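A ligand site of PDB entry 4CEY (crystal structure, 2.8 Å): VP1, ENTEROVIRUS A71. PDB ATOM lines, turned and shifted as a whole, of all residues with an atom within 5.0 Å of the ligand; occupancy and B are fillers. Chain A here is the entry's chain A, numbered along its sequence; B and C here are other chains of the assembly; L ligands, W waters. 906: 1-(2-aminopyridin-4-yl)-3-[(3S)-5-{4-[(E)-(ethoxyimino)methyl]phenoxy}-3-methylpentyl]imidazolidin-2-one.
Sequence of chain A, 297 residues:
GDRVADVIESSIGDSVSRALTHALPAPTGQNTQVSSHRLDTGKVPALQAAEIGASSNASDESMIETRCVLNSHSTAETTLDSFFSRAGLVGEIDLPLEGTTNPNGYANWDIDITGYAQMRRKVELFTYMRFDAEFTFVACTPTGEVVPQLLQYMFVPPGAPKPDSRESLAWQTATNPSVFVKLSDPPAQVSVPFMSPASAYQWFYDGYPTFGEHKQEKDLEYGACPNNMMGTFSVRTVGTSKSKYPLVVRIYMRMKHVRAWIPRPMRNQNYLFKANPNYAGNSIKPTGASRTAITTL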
ATOM      1  N   ILE A 111      12.734  -0.990  -7.058  1.00  0.00           N
ATOM      2  CA  ILE A 111      12.780  -0.408  -5.741  1.00  0.00           C
ATOM      3  C   ILE A 111      12.559   1.093  -5.823  1.00  0.00           C
ATOM      4  O   ILE A 111      13.450   1.851  -6.180  1.00  0.00           O
ATOM      5  CB  ILE A 111      14.096  -0.742  -5.071  1.00  0.00           C
ATOM      6  CG1 ILE A 111      14.324  -2.261  -5.161  1.00  0.00           C
ATOM      7  CG2 ILE A 111      14.033  -0.373  -3.613  1.00  0.00           C
ATOM      8  CD1 ILE A 111      15.593  -2.743  -4.483  1.00  0.00           C
ATOM      9  N   ASP A 112      11.327   1.494  -5.505  1.00  0.00           N
ATOM     10  CA  ASP A 112      10.901   2.874  -5.553  1.00  0.00           C
ATOM     11  C   ASP A 112       9.769   2.961  -4.541  1.00  0.00           C
ATOM     12  O   ASP A 112       8.701   2.357  -4.717  1.00  0.00           O
ATOM     13  CB  ASP A 112      10.400   3.184  -6.966  1.00  0.00           C
ATOM     14  CG  ASP A 112       9.982   4.607  -7.140  1.00  0.00           C
ATOM     15  OD1 ASP A 112       9.633   5.255  -6.136  1.00  0.00           O
ATOM     16  OD2 ASP A 112       9.987   5.079  -8.298  1.00  0.00           O
ATOM     17  N   ILE A 113       9.982   3.690  -3.461  1.00  0.00           N
ATOM     18  CA  ILE A 113       8.958   3.777  -2.426  1.00  0.00           C
ATOM     19  C   ILE A 113       7.944   4.906  -2.599  1.00  0.00           C
ATOM     20  O   ILE A 113       7.175   5.161  -1.687  1.00  0.00           O
ATOM     21  CB  ILE A 113       9.577   3.966  -1.043  1.00  0.00           C
ATOM     22  CG1 ILE A 113      10.269   5.320  -1.014  1.00  0.00           C
ATOM     23  CG2 ILE A 113      10.580   2.870  -0.749  1.00  0.00           C
ATOM     24  CD1 ILE A 113      10.322   5.912   0.342  1.00  0.00           C
ATOM     25  N   THR A 114       7.926   5.564  -3.750  1.00  0.00           N
ATOM     26  CA  THR A 114       7.002   6.670  -3.937  1.00  0.00           C
ATOM     27  C   THR A 114       5.596   6.317  -4.405  1.00  0.00           C
ATOM     28  O   THR A 114       4.834   7.203  -4.780  1.00  0.00           O
ATOM     29  CB  THR A 114       7.559   7.689  -4.914  1.00  0.00           C
ATOM     30  OG1 THR A 114       7.829   7.041  -6.155  1.00  0.00           O
ATOM     31  CG2 THR A 114       8.829   8.281  -4.398  1.00  0.00           C
ATOM     32  N   PHE A 131      20.128   7.248   5.184  1.00  0.00           N
ATOM     33  CA  PHE A 131      19.648   6.360   6.224  1.00  0.00           C
ATOM     34  C   PHE A 131      19.834   4.887   5.904  1.00  0.00           C
ATOM     35  O   PHE A 131      20.112   4.511   4.780  1.00  0.00           O
ATOM     36  CB  PHE A 131      18.157   6.640   6.482  1.00  0.00           C
ATOM     37  CG  PHE A 131      17.292   6.485   5.257  1.00  0.00           C
ATOM     38  CD1 PHE A 131      16.799   5.237   4.874  1.00  0.00           C
ATOM     39  CD2 PHE A 131      17.001   7.590   4.456  1.00  0.00           C
ATOM     40  CE1 PHE A 131      16.041   5.092   3.708  1.00  0.00           C
ATOM     41  CE2 PHE A 131      16.254   7.449   3.285  1.00  0.00           C
ATOM     42  CZ  PHE A 131      15.768   6.198   2.914  1.00  0.00           C
ATOM     43  N   ALA A 133      17.957   1.041   6.598  1.00  0.00           N
ATOM     44  CA  ALA A 133      16.552   0.688   6.654  1.00  0.00           C
ATOM     45  C   ALA A 133      16.339  -0.775   6.948  1.00  0.00           C
ATOM     46  O   ALA A 133      17.159  -1.625   6.585  1.00  0.00           O
ATOM     47  CB  ALA A 133      15.871   1.033   5.330  1.00  0.00           C
ATOM     48  N   PHE A 135      13.731  -3.772   6.280  1.00  0.00           N
ATOM     49  CA  PHE A 135      12.628  -4.162   5.426  1.00  0.00           C
ATOM     50  C   PHE A 135      11.933  -5.430   5.919  1.00  0.00           C
ATOM     51  O   PHE A 135      12.590  -6.415   6.279  1.00  0.00           O
ATOM     52  CB  PHE A 135      13.099  -4.324   3.975  1.00  0.00           C
ATOM     53  CG  PHE A 135      13.125  -3.026   3.203  1.00  0.00           C
ATOM     54  CD1 PHE A 135      14.090  -2.061   3.461  1.00  0.00           C
ATOM     55  CD2 PHE A 135      12.148  -2.749   2.262  1.00  0.00           C
ATOM     56  CE1 PHE A 135      14.072  -0.826   2.796  1.00  0.00           C
ATOM     57  CE2 PHE A 135      12.121  -1.514   1.594  1.00  0.00           C
ATOM     58  CZ  PHE A 135      13.083  -0.553   1.861  1.00  0.00           C
ATOM     59  N   PHE A 137       8.800  -8.240   5.022  1.00  0.00           N
ATOM     60  CA  PHE A 137       7.941  -8.791   3.973  1.00  0.00           C
ATOM     61  C   PHE A 137       6.826  -9.668   4.514  1.00  0.00           C
ATOM     62  O   PHE A 137       7.077 -10.748   5.055  1.00  0.00           O
ATOM     63  CB  PHE A 137       8.797  -9.585   2.996  1.00  0.00           C
ATOM     64  CG  PHE A 137       9.980  -8.815   2.491  1.00  0.00           C
ATOM     65  CD1 PHE A 137       9.823  -7.828   1.532  1.00  0.00           C
ATOM     66  CD2 PHE A 137      11.233  -9.026   3.043  1.00  0.00           C
ATOM     67  CE1 PHE A 137      10.909  -7.043   1.126  1.00  0.00           C
ATOM     68  CE2 PHE A 137      12.323  -8.247   2.657  1.00  0.00           C
ATOM     69  CZ  PHE A 137      12.169  -7.256   1.690  1.00  0.00           C
ATOM     70  N   TYR A 153      13.106 -14.477  -2.250  1.00  0.00           N
ATOM     71  CA  TYR A 153      13.221 -13.046  -2.531  1.00  0.00           C
ATOM     72  C   TYR A 153      14.698 -12.857  -2.895  1.00  0.00           C
ATOM     73  O   TYR A 153      15.586 -13.433  -2.262  1.00  0.00           O
ATOM     74  CB  TYR A 153      12.917 -12.191  -1.289  1.00  0.00           C
ATOM     75  CG  TYR A 153      11.572 -12.423  -0.621  1.00  0.00           C
ATOM     76  CD1 TYR A 153      10.402 -12.542  -1.361  1.00  0.00           C
ATOM     77  CD2 TYR A 153      11.466 -12.485   0.760  1.00  0.00           C
ATOM     78  CE1 TYR A 153       9.166 -12.708  -0.745  1.00  0.00           C
ATOM     79  CE2 TYR A 153      10.236 -12.653   1.388  1.00  0.00           C
ATOM     80  CZ  TYR A 153       9.094 -12.761   0.628  1.00  0.00           C
ATOM     81  OH  TYR A 153       7.877 -12.925   1.251  1.00  0.00           O
ATOM     82  N   MET A 154      14.969 -12.062  -3.924  1.00  0.00           N
ATOM     83  CA  MET A 154      16.353 -11.832  -4.302  1.00  0.00           C
ATOM     84  C   MET A 154      16.549 -10.392  -4.698  1.00  0.00           C
ATOM     85  O   MET A 154      15.745  -9.826  -5.420  1.00  0.00           O
ATOM     86  CB  MET A 154      16.766 -12.741  -5.451  1.00  0.00           C
ATOM     87  CG  MET A 154      18.113 -12.369  -6.055  1.00  0.00           C
ATOM     88  SD  MET A 154      18.723 -13.621  -7.193  1.00  0.00           S
ATOM     89  CE  MET A 154      17.891 -13.151  -8.751  1.00  0.00           C
ATOM     90  N   PHE A 155      17.612  -9.787  -4.199  1.00  0.00           N
ATOM     91  CA  PHE A 155      17.921  -8.397  -4.512  1.00  0.00           C
ATOM     92  C   PHE A 155      18.877  -8.402  -5.705  1.00  0.00           C
ATOM     93  O   PHE A 155      19.946  -8.988  -5.666  1.00  0.00           O
ATOM     94  CB  PHE A 155      18.539  -7.735  -3.274  1.00  0.00           C
ATOM     95  CG  PHE A 155      19.106  -6.362  -3.534  1.00  0.00           C
ATOM     96  CD1 PHE A 155      18.455  -5.469  -4.361  1.00  0.00           C
ATOM     97  CD2 PHE A 155      20.309  -5.977  -2.940  1.00  0.00           C
ATOM     98  CE1 PHE A 155      18.998  -4.205  -4.625  1.00  0.00           C
ATOM     99  CE2 PHE A 155      20.850  -4.725  -3.198  1.00  0.00           C
ATOM    100  CZ  PHE A 155      20.192  -3.843  -4.032  1.00  0.00           C
ATOM    101  N   PRO A 177      22.112 -11.173  -2.783  1.00  0.00           N
ATOM    102  CA  PRO A 177      21.617 -11.758  -1.534  1.00  0.00           C
ATOM    103  C   PRO A 177      20.170 -12.249  -1.732  1.00  0.00           C
ATOM    104  O   PRO A 177      19.333 -11.528  -2.293  1.00  0.00           O
ATOM    105  CB  PRO A 177      21.728 -10.603  -0.538  1.00  0.00           C
ATOM    106  CG  PRO A 177      21.505  -9.402  -1.403  1.00  0.00           C
ATOM    107  CD  PRO A 177      22.318  -9.722  -2.649  1.00  0.00           C
ATOM    108  N   SER A 178      19.878 -13.480  -1.309  1.00  0.00           N
ATOM    109  CA  SER A 178      18.514 -14.023  -1.434  1.00  0.00           C
ATOM    110  C   SER A 178      17.976 -14.422  -0.060  1.00  0.00           C
ATOM    111  O   SER A 178      18.730 -14.671   0.876  1.00  0.00           O
ATOM    112  CB  SER A 178      18.495 -15.277  -2.338  1.00  0.00           C
ATOM    113  OG  SER A 178      18.523 -14.951  -3.723  1.00  0.00           O
ATOM    114  N   VAL A 179      16.655 -14.454   0.066  1.00  0.00           N
ATOM    115  CA  VAL A 179      16.026 -14.889   1.308  1.00  0.00           C
ATOM    116  C   VAL A 179      15.033 -15.981   0.937  1.00  0.00           C
ATOM    117  O   VAL A 179      14.221 -15.792   0.026  1.00  0.00           O
ATOM    118  CB  VAL A 179      15.247 -13.765   2.032  1.00  0.00           C
ATOM    119  CG1 VAL A 179      14.421 -14.371   3.170  1.00  0.00           C
ATOM    120  CG2 VAL A 179      16.189 -12.721   2.592  1.00  0.00           C
ATOM    121  N   VAL A 190      15.042  -7.985   7.121  1.00  0.00           N
ATOM    122  CA  VAL A 190      16.480  -7.762   6.992  1.00  0.00           C
ATOM    123  C   VAL A 190      16.850  -6.298   7.106  1.00  0.00           C
ATOM    124  O   VAL A 190      15.987  -5.420   7.064  1.00  0.00           O
ATOM    125  CB  VAL A 190      17.000  -8.293   5.618  1.00  0.00           C
ATOM    126  CG1 VAL A 190      16.621  -9.757   5.468  1.00  0.00           C
ATOM    127  CG2 VAL A 190      16.422  -7.486   4.468  1.00  0.00           C
ATOM    128  N   VAL A 192      19.114  -3.140   5.583  1.00  0.00           N
ATOM    129  CA  VAL A 192      19.676  -2.652   4.340  1.00  0.00           C
ATOM    130  C   VAL A 192      20.488  -1.402   4.658  1.00  0.00           C
ATOM    131  O   VAL A 192      20.028  -0.525   5.390  1.00  0.00           O
ATOM    132  CB  VAL A 192      18.542  -2.289   3.349  1.00  0.00           C
ATOM    133  CG1 VAL A 192      19.100  -1.785   2.054  1.00  0.00           C
ATOM    134  CG2 VAL A 192      17.684  -3.516   3.103  1.00  0.00           C
ATOM    135  N   MET A 195      22.954   2.591   0.338  1.00  0.00           N
ATOM    136  CA  MET A 195      23.673   2.154  -0.860  1.00  0.00           C
ATOM    137  C   MET A 195      23.938   3.099  -2.024  1.00  0.00           C
ATOM    138  O   MET A 195      24.542   2.692  -3.013  1.00  0.00           O
ATOM    139  CB  MET A 195      22.987   0.911  -1.425  1.00  0.00           C
ATOM    140  CG  MET A 195      22.702  -0.186  -0.392  1.00  0.00           C
ATOM    141  SD  MET A 195      21.668  -1.495  -1.070  1.00  0.00           S
ATOM    142  CE  MET A 195      20.082  -0.748  -0.956  1.00  0.00           C
ATOM    143  N   TYR A 201      20.371  10.243  -0.542  1.00  0.00           N
ATOM    144  CA  TYR A 201      19.365   9.996  -1.557  1.00  0.00           C
ATOM    145  C   TYR A 201      18.728  11.383  -1.669  1.00  0.00           C
ATOM    146  O   TYR A 201      18.844  12.180  -0.751  1.00  0.00           O
ATOM    147  CB  TYR A 201      18.299   9.021  -1.048  1.00  0.00           C
ATOM    148  CG  TYR A 201      18.722   7.595  -0.796  1.00  0.00           C
ATOM    149  CD1 TYR A 201      19.328   6.839  -1.792  1.00  0.00           C
ATOM    150  CD2 TYR A 201      18.456   6.979   0.437  1.00  0.00           C
ATOM    151  CE1 TYR A 201      19.665   5.496  -1.580  1.00  0.00           C
ATOM    152  CE2 TYR A 201      18.787   5.652   0.665  1.00  0.00           C
ATOM    153  CZ  TYR A 201      19.395   4.909  -0.338  1.00  0.00           C
ATOM    154  OH  TYR A 201      19.750   3.590  -0.122  1.00  0.00           O
ATOM    155  N   GLN A 202      18.071  11.684  -2.778  1.00  0.00           N
ATOM    156  CA  GLN A 202      17.393  12.964  -2.877  1.00  0.00           C
ATOM    157  C   GLN A 202      16.060  12.720  -3.549  1.00  0.00           C
ATOM    158  O   GLN A 202      15.995  12.075  -4.583  1.00  0.00           O
ATOM    159  CB  GLN A 202      18.227  13.983  -3.644  1.00  0.00           C
ATOM    160  CG  GLN A 202      18.332  13.826  -5.108  1.00  0.00           C
ATOM    161  CD  GLN A 202      19.420  14.714  -5.665  1.00  0.00           C
ATOM    162  OE1 GLN A 202      20.572  14.295  -5.804  1.00  0.00           O
ATOM    163  NE2 GLN A 202      19.075  15.964  -5.960  1.00  0.00           N
ATOM    164  N   TRP A 203      14.983  13.208  -2.925  1.00  0.00           N
ATOM    165  CA  TRP A 203      13.633  13.025  -3.433  1.00  0.00           C
ATOM    166  C   TRP A 203      13.270  13.978  -4.559  1.00  0.00           C
ATOM    167  O   TRP A 203      12.194  13.877  -5.140  1.00  0.00           O
ATOM    168  CB  TRP A 203      12.622  13.197  -2.295  1.00  0.00           C
ATOM    169  CG  TRP A 203      12.902  12.290  -1.122  1.00  0.00           C
ATOM    170  CD1 TRP A 203      13.392  12.656   0.109  1.00  0.00           C
ATOM    171  CD2 TRP A 203      12.789  10.857  -1.097  1.00  0.00           C
ATOM    172  NE1 TRP A 203      13.596  11.543   0.890  1.00  0.00           N
ATOM    173  CE2 TRP A 203      13.239  10.425   0.176  1.00  0.00           C
ATOM    174  CE3 TRP A 203      12.356   9.900  -2.020  1.00  0.00           C
ATOM    175  CZ2 TRP A 203      13.269   9.075   0.544  1.00  0.00           C
ATOM    176  CZ3 TRP A 203      12.386   8.550  -1.652  1.00  0.00           C
ATOM    177  CH2 TRP A 203      12.837   8.153  -0.388  1.00  0.00           C
ATOM    178  N   ASN A 228      19.422   7.377  -7.113  1.00  0.00           N
ATOM    179  CA  ASN A 228      18.289   6.948  -6.285  1.00  0.00           C
ATOM    180  C   ASN A 228      17.762   5.599  -6.706  1.00  0.00           C
ATOM    181  O   ASN A 228      16.880   5.028  -6.065  1.00  0.00           O
ATOM    182  CB  ASN A 228      17.132   7.944  -6.387  1.00  0.00           C
ATOM    183  CG  ASN A 228      17.457   9.305  -5.780  1.00  0.00           C
ATOM    184  OD1 ASN A 228      18.090   9.392  -4.732  1.00  0.00           O
ATOM    185  ND2 ASN A 228      16.989  10.372  -6.428  1.00  0.00           N
ATOM    186  N   MET A 230      18.263   2.009  -6.768  1.00  0.00           N
ATOM    187  CA  MET A 230      19.028   0.950  -6.123  1.00  0.00           C
ATOM    188  C   MET A 230      18.909  -0.445  -6.677  1.00  0.00           C
ATOM    189  O   MET A 230      19.616  -1.341  -6.235  1.00  0.00           O
ATOM    190  CB  MET A 230      18.716   0.939  -4.643  1.00  0.00           C
ATOM    191  CG  MET A 230      19.104   2.243  -3.960  1.00  0.00           C
ATOM    192  SD  MET A 230      20.881   2.562  -4.078  1.00  0.00           S
ATOM    193  CE  MET A 230      20.989   3.612  -5.453  1.00  0.00           C
ATOM    194  N   PHE A 233      13.845  -5.874  -6.880  1.00  0.00           N
ATOM    195  CA  PHE A 233      13.527  -6.866  -5.862  1.00  0.00           C
ATOM    196  C   PHE A 233      12.721  -7.935  -6.600  1.00  0.00           C
ATOM    197  O   PHE A 233      11.635  -7.661  -7.097  1.00  0.00           O
ATOM    198  CB  PHE A 233      12.645  -6.261  -4.775  1.00  0.00           C
ATOM    199  CG  PHE A 233      12.337  -7.192  -3.641  1.00  0.00           C
ATOM    200  CD1 PHE A 233      13.328  -7.554  -2.728  1.00  0.00           C
ATOM    201  CD2 PHE A 233      11.046  -7.707  -3.487  1.00  0.00           C
ATOM    202  CE1 PHE A 233      13.042  -8.414  -1.672  1.00  0.00           C
ATOM    203  CE2 PHE A 233      10.762  -8.576  -2.434  1.00  0.00           C
ATOM    204  CZ  PHE A 233      11.751  -8.928  -1.518  1.00  0.00           C
ATOM    205  N   MET A 253       8.778  -0.679   5.210  1.00  0.00           N
ATOM    206  CA  MET A 253      10.092  -0.095   5.413  1.00  0.00           C
ATOM    207  C   MET A 253      10.183   0.712   6.684  1.00  0.00           C
ATOM    208  O   MET A 253       9.320   1.541   6.991  1.00  0.00           O
ATOM    209  CB  MET A 253      10.470   0.809   4.235  1.00  0.00           C
ATOM    210  CG  MET A 253      11.776   1.554   4.463  1.00  0.00           C
ATOM    211  SD  MET A 253      12.205   2.747   3.177  1.00  0.00           S
ATOM    212  CE  MET A 253      11.186   4.155   3.654  1.00  0.00           C
ATOM    213  N   LYS A 274       4.657   8.273  -9.583  1.00  0.00           N
ATOM    214  CA  LYS A 274       5.814   8.048  -8.744  1.00  0.00           C
ATOM    215  C   LYS A 274       6.966   8.952  -9.118  1.00  0.00           C
ATOM    216  O   LYS A 274       7.598   9.557  -8.254  1.00  0.00           O
ATOM    217  CB  LYS A 274       6.313   6.619  -8.870  1.00  0.00           C
ATOM    218  CG  LYS A 274       5.332   5.556  -8.568  1.00  0.00           C
ATOM    219  CD  LYS A 274       6.062   4.258  -8.649  1.00  0.00           C
ATOM    220  CE  LYS A 274       5.131   3.111  -8.821  1.00  0.00           C
ATOM    221  NZ  LYS A 274       5.942   1.901  -8.999  1.00  0.00           N
ATOM    222  N   ILE B  24      21.960  -7.659   4.888  1.00  0.00           N
ATOM    223  CA  ILE B  24      22.049  -8.308   3.589  1.00  0.00           C
ATOM    224  C   ILE B  24      23.397  -8.243   2.881  1.00  0.00           C
ATOM    225  O   ILE B  24      23.729  -9.157   2.128  1.00  0.00           O
ATOM    226  CB  ILE B  24      21.007  -7.763   2.606  1.00  0.00           C
ATOM    227  CG1 ILE B  24      21.276  -6.297   2.332  1.00  0.00           C
ATOM    228  CG2 ILE B  24      19.597  -7.976   3.149  1.00  0.00           C
ATOM    229  CD1 ILE B  24      20.519  -5.783   1.137  1.00  0.00           C
ATOM    230  N   LEU C  14      18.790 -16.460   4.813  1.00  0.00           N
ATOM    231  CA  LEU C  14      19.370 -15.352   4.033  1.00  0.00           C
ATOM    232  C   LEU C  14      20.729 -15.845   3.575  1.00  0.00           C
ATOM    233  O   LEU C  14      21.608 -16.112   4.400  1.00  0.00           O
ATOM    234  CB  LEU C  14      19.503 -14.103   4.916  1.00  0.00           C
ATOM    235  CG  LEU C  14      20.300 -12.898   4.409  1.00  0.00           C
ATOM    236  CD1 LEU C  14      19.559 -12.193   3.292  1.00  0.00           C
ATOM    237  CD2 LEU C  14      20.517 -11.924   5.560  1.00  0.00           C
HETATM  238  CAA 906 L   1      16.879 -10.872   0.143  1.00  0.00           C
HETATM  239  CAB 906 L   1      15.960   2.189   1.190  1.00  0.00           C
HETATM  240  NAC 906 L   1      11.003   7.838  -7.044  1.00  0.00           N
HETATM  241  OAD 906 L   1      12.839   5.235  -3.800  1.00  0.00           O
HETATM  242  CAE 906 L   1      15.818  -6.244   0.453  1.00  0.00           C
HETATM  243  CAF 906 L   1      13.625   9.923  -5.758  1.00  0.00           C
HETATM  244  CAG 906 L   1      14.198   9.095  -4.808  1.00  0.00           C
HETATM  245  CAH 906 L   1      15.246  -3.913   0.418  1.00  0.00           C
HETATM  246  CAI 906 L   1      17.075  -4.708  -0.932  1.00  0.00           C
HETATM  247  CAJ 906 L   1      15.480  -2.619  -0.034  1.00  0.00           C
HETATM  248  CAK 906 L   1      17.299  -3.415  -1.386  1.00  0.00           C
HETATM  249  CAL 906 L   1      12.586   7.404  -5.368  1.00  0.00           C
HETATM  250  CAM 906 L   1      17.340  -9.439  -0.128  1.00  0.00           C
HETATM  251  CAN 906 L   1      16.017  -0.153  -0.525  1.00  0.00           C
HETATM  252  CAO 906 L   1      16.146   1.256  -1.122  1.00  0.00           C
HETATM  253  CAP 906 L   1      15.482   3.649  -0.773  1.00  0.00           C
HETATM  254  CAQ 906 L   1      14.589   3.800  -2.003  1.00  0.00           C
HETATM  255  CAR 906 L   1      15.906   6.032  -2.380  1.00  0.00           C
HETATM  256  CAS 906 L   1      15.351   7.390  -2.823  1.00  0.00           C
HETATM  257  NAT 906 L   1      16.657  -7.185   0.018  1.00  0.00           N
HETATM  258  NAU 906 L   1      12.534   9.482  -6.516  1.00  0.00           N
HETATM  259  OAV 906 L   1      16.422  -8.536   0.514  1.00  0.00           O
HETATM  260  OAW 906 L   1      16.828  -1.078  -1.253  1.00  0.00           O
HETATM  261  CAX 906 L   1      13.884   5.757  -3.416  1.00  0.00           C
HETATM  262  CAY 906 L   1      12.033   8.246  -6.317  1.00  0.00           C
HETATM  263  CAZ 906 L   1      16.042  -4.964  -0.028  1.00  0.00           C
HETATM  264  CBA 906 L   1      16.501  -2.354  -0.937  1.00  0.00           C
HETATM  265  CBB 906 L   1      13.665   7.818  -4.601  1.00  0.00           C
HETATM  266  CBC 906 L   1      15.378   2.227  -0.218  1.00  0.00           C
HETATM  267  NBD 906 L   1      14.723   5.158  -2.573  1.00  0.00           N
HETATM  268  NBE 906 L   1      14.259   6.992  -3.744  1.00  0.00           N
HETATM  269  O   HOH W   1      10.013  10.827  -7.521  1.00  0.00           O
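Ile 111 touches the ligand.
CE1 of Phe 131 touches CAB of the ligand (3.8 Å).
Phe 135 touches the ligand.
Phe 137 touches the ligand.
Tyr 153 touches the ligand (O to CAA, 3.7 Å).
CG of Phe 155 touches CAI of the ligand (3.7 Å).
O of Pro 177 touches CAA of the ligand, 3.5 Å away.
Ser 178 touches the ligand (C to CAA, 3.7 Å).
Val 179 touches the ligand.
Val 192 touches the ligand (CG2 to CAH, 3.6 Å).
Met 195 touches the ligand.
Tyr 201 touches the ligand.
Gln 202 touches the ligand (O to CAF, 3.4 Å).
Trp 203 touches the ligand (CZ3 to NBE, 3.2 Å).
Asn 228 touches the ligand (CG to CAG, 3.4 Å).
Within 4 Å of the ligand: Ile 111, Asp 112, Ile 113, Thr 114, Phe 131, Phe 135, Phe 137, Tyr 153, Phe 155, Pro 177, Ser 178, Val 179, Val 192, Met 195, Tyr 201, Gln 202, Trp 203 and Asn 228.
The side-chain hydroxyl of Thr 114 sits close to the backbone carbonyl oxygen of Lys 274.
The side-chain carboxylate of Asp 112 lies within hydrogen-bond range of the side-chain hydroxyl of Thr 114.
The backbone NH (N) of Val 192 is in hydrogen-bond range of the backbone carbonyl oxygen (O) of Ala 133, 2.7 Å away.
The side-chain amide nitrogen (ND2) of Asn 228 sits at hydrogen-bond distance from the backbone carbonyl oxygen (O) of Gln 202 (2.7 Å).
The backbone NH (N) of Met 195 sits at hydrogen-bond distance from the side-chain hydroxyl (OH) of Tyr 201 (3.4 Å).
O of Pro 177 sits at hydrogen-bond distance from N of Phe 155.
The side-chain hydroxyl (OG) of Ser 178 sits close to the side-chain sulfur (SD) of Met 154, 3.7 Å away.
N of Val 179 is in hydrogen-bond range of O of Tyr 153 (2.8 Å).
OD1 of Asp 112 is in hydrogen-bond range of NAC of the ligand (3.1 Å).
N of Ile 113 sits at hydrogen-bond distance from OAD of the ligand, 3.3 Å away.
A nitrogen (NAC) of the ligand is in hydrogen-bond range of the side-chain hydroxyl of Thr 114 (3.4 Å).
Water W1 lies within hydrogen-bond range of O of Lys 274 (2.8 Å) and NAU of the ligand (3.0 Å).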
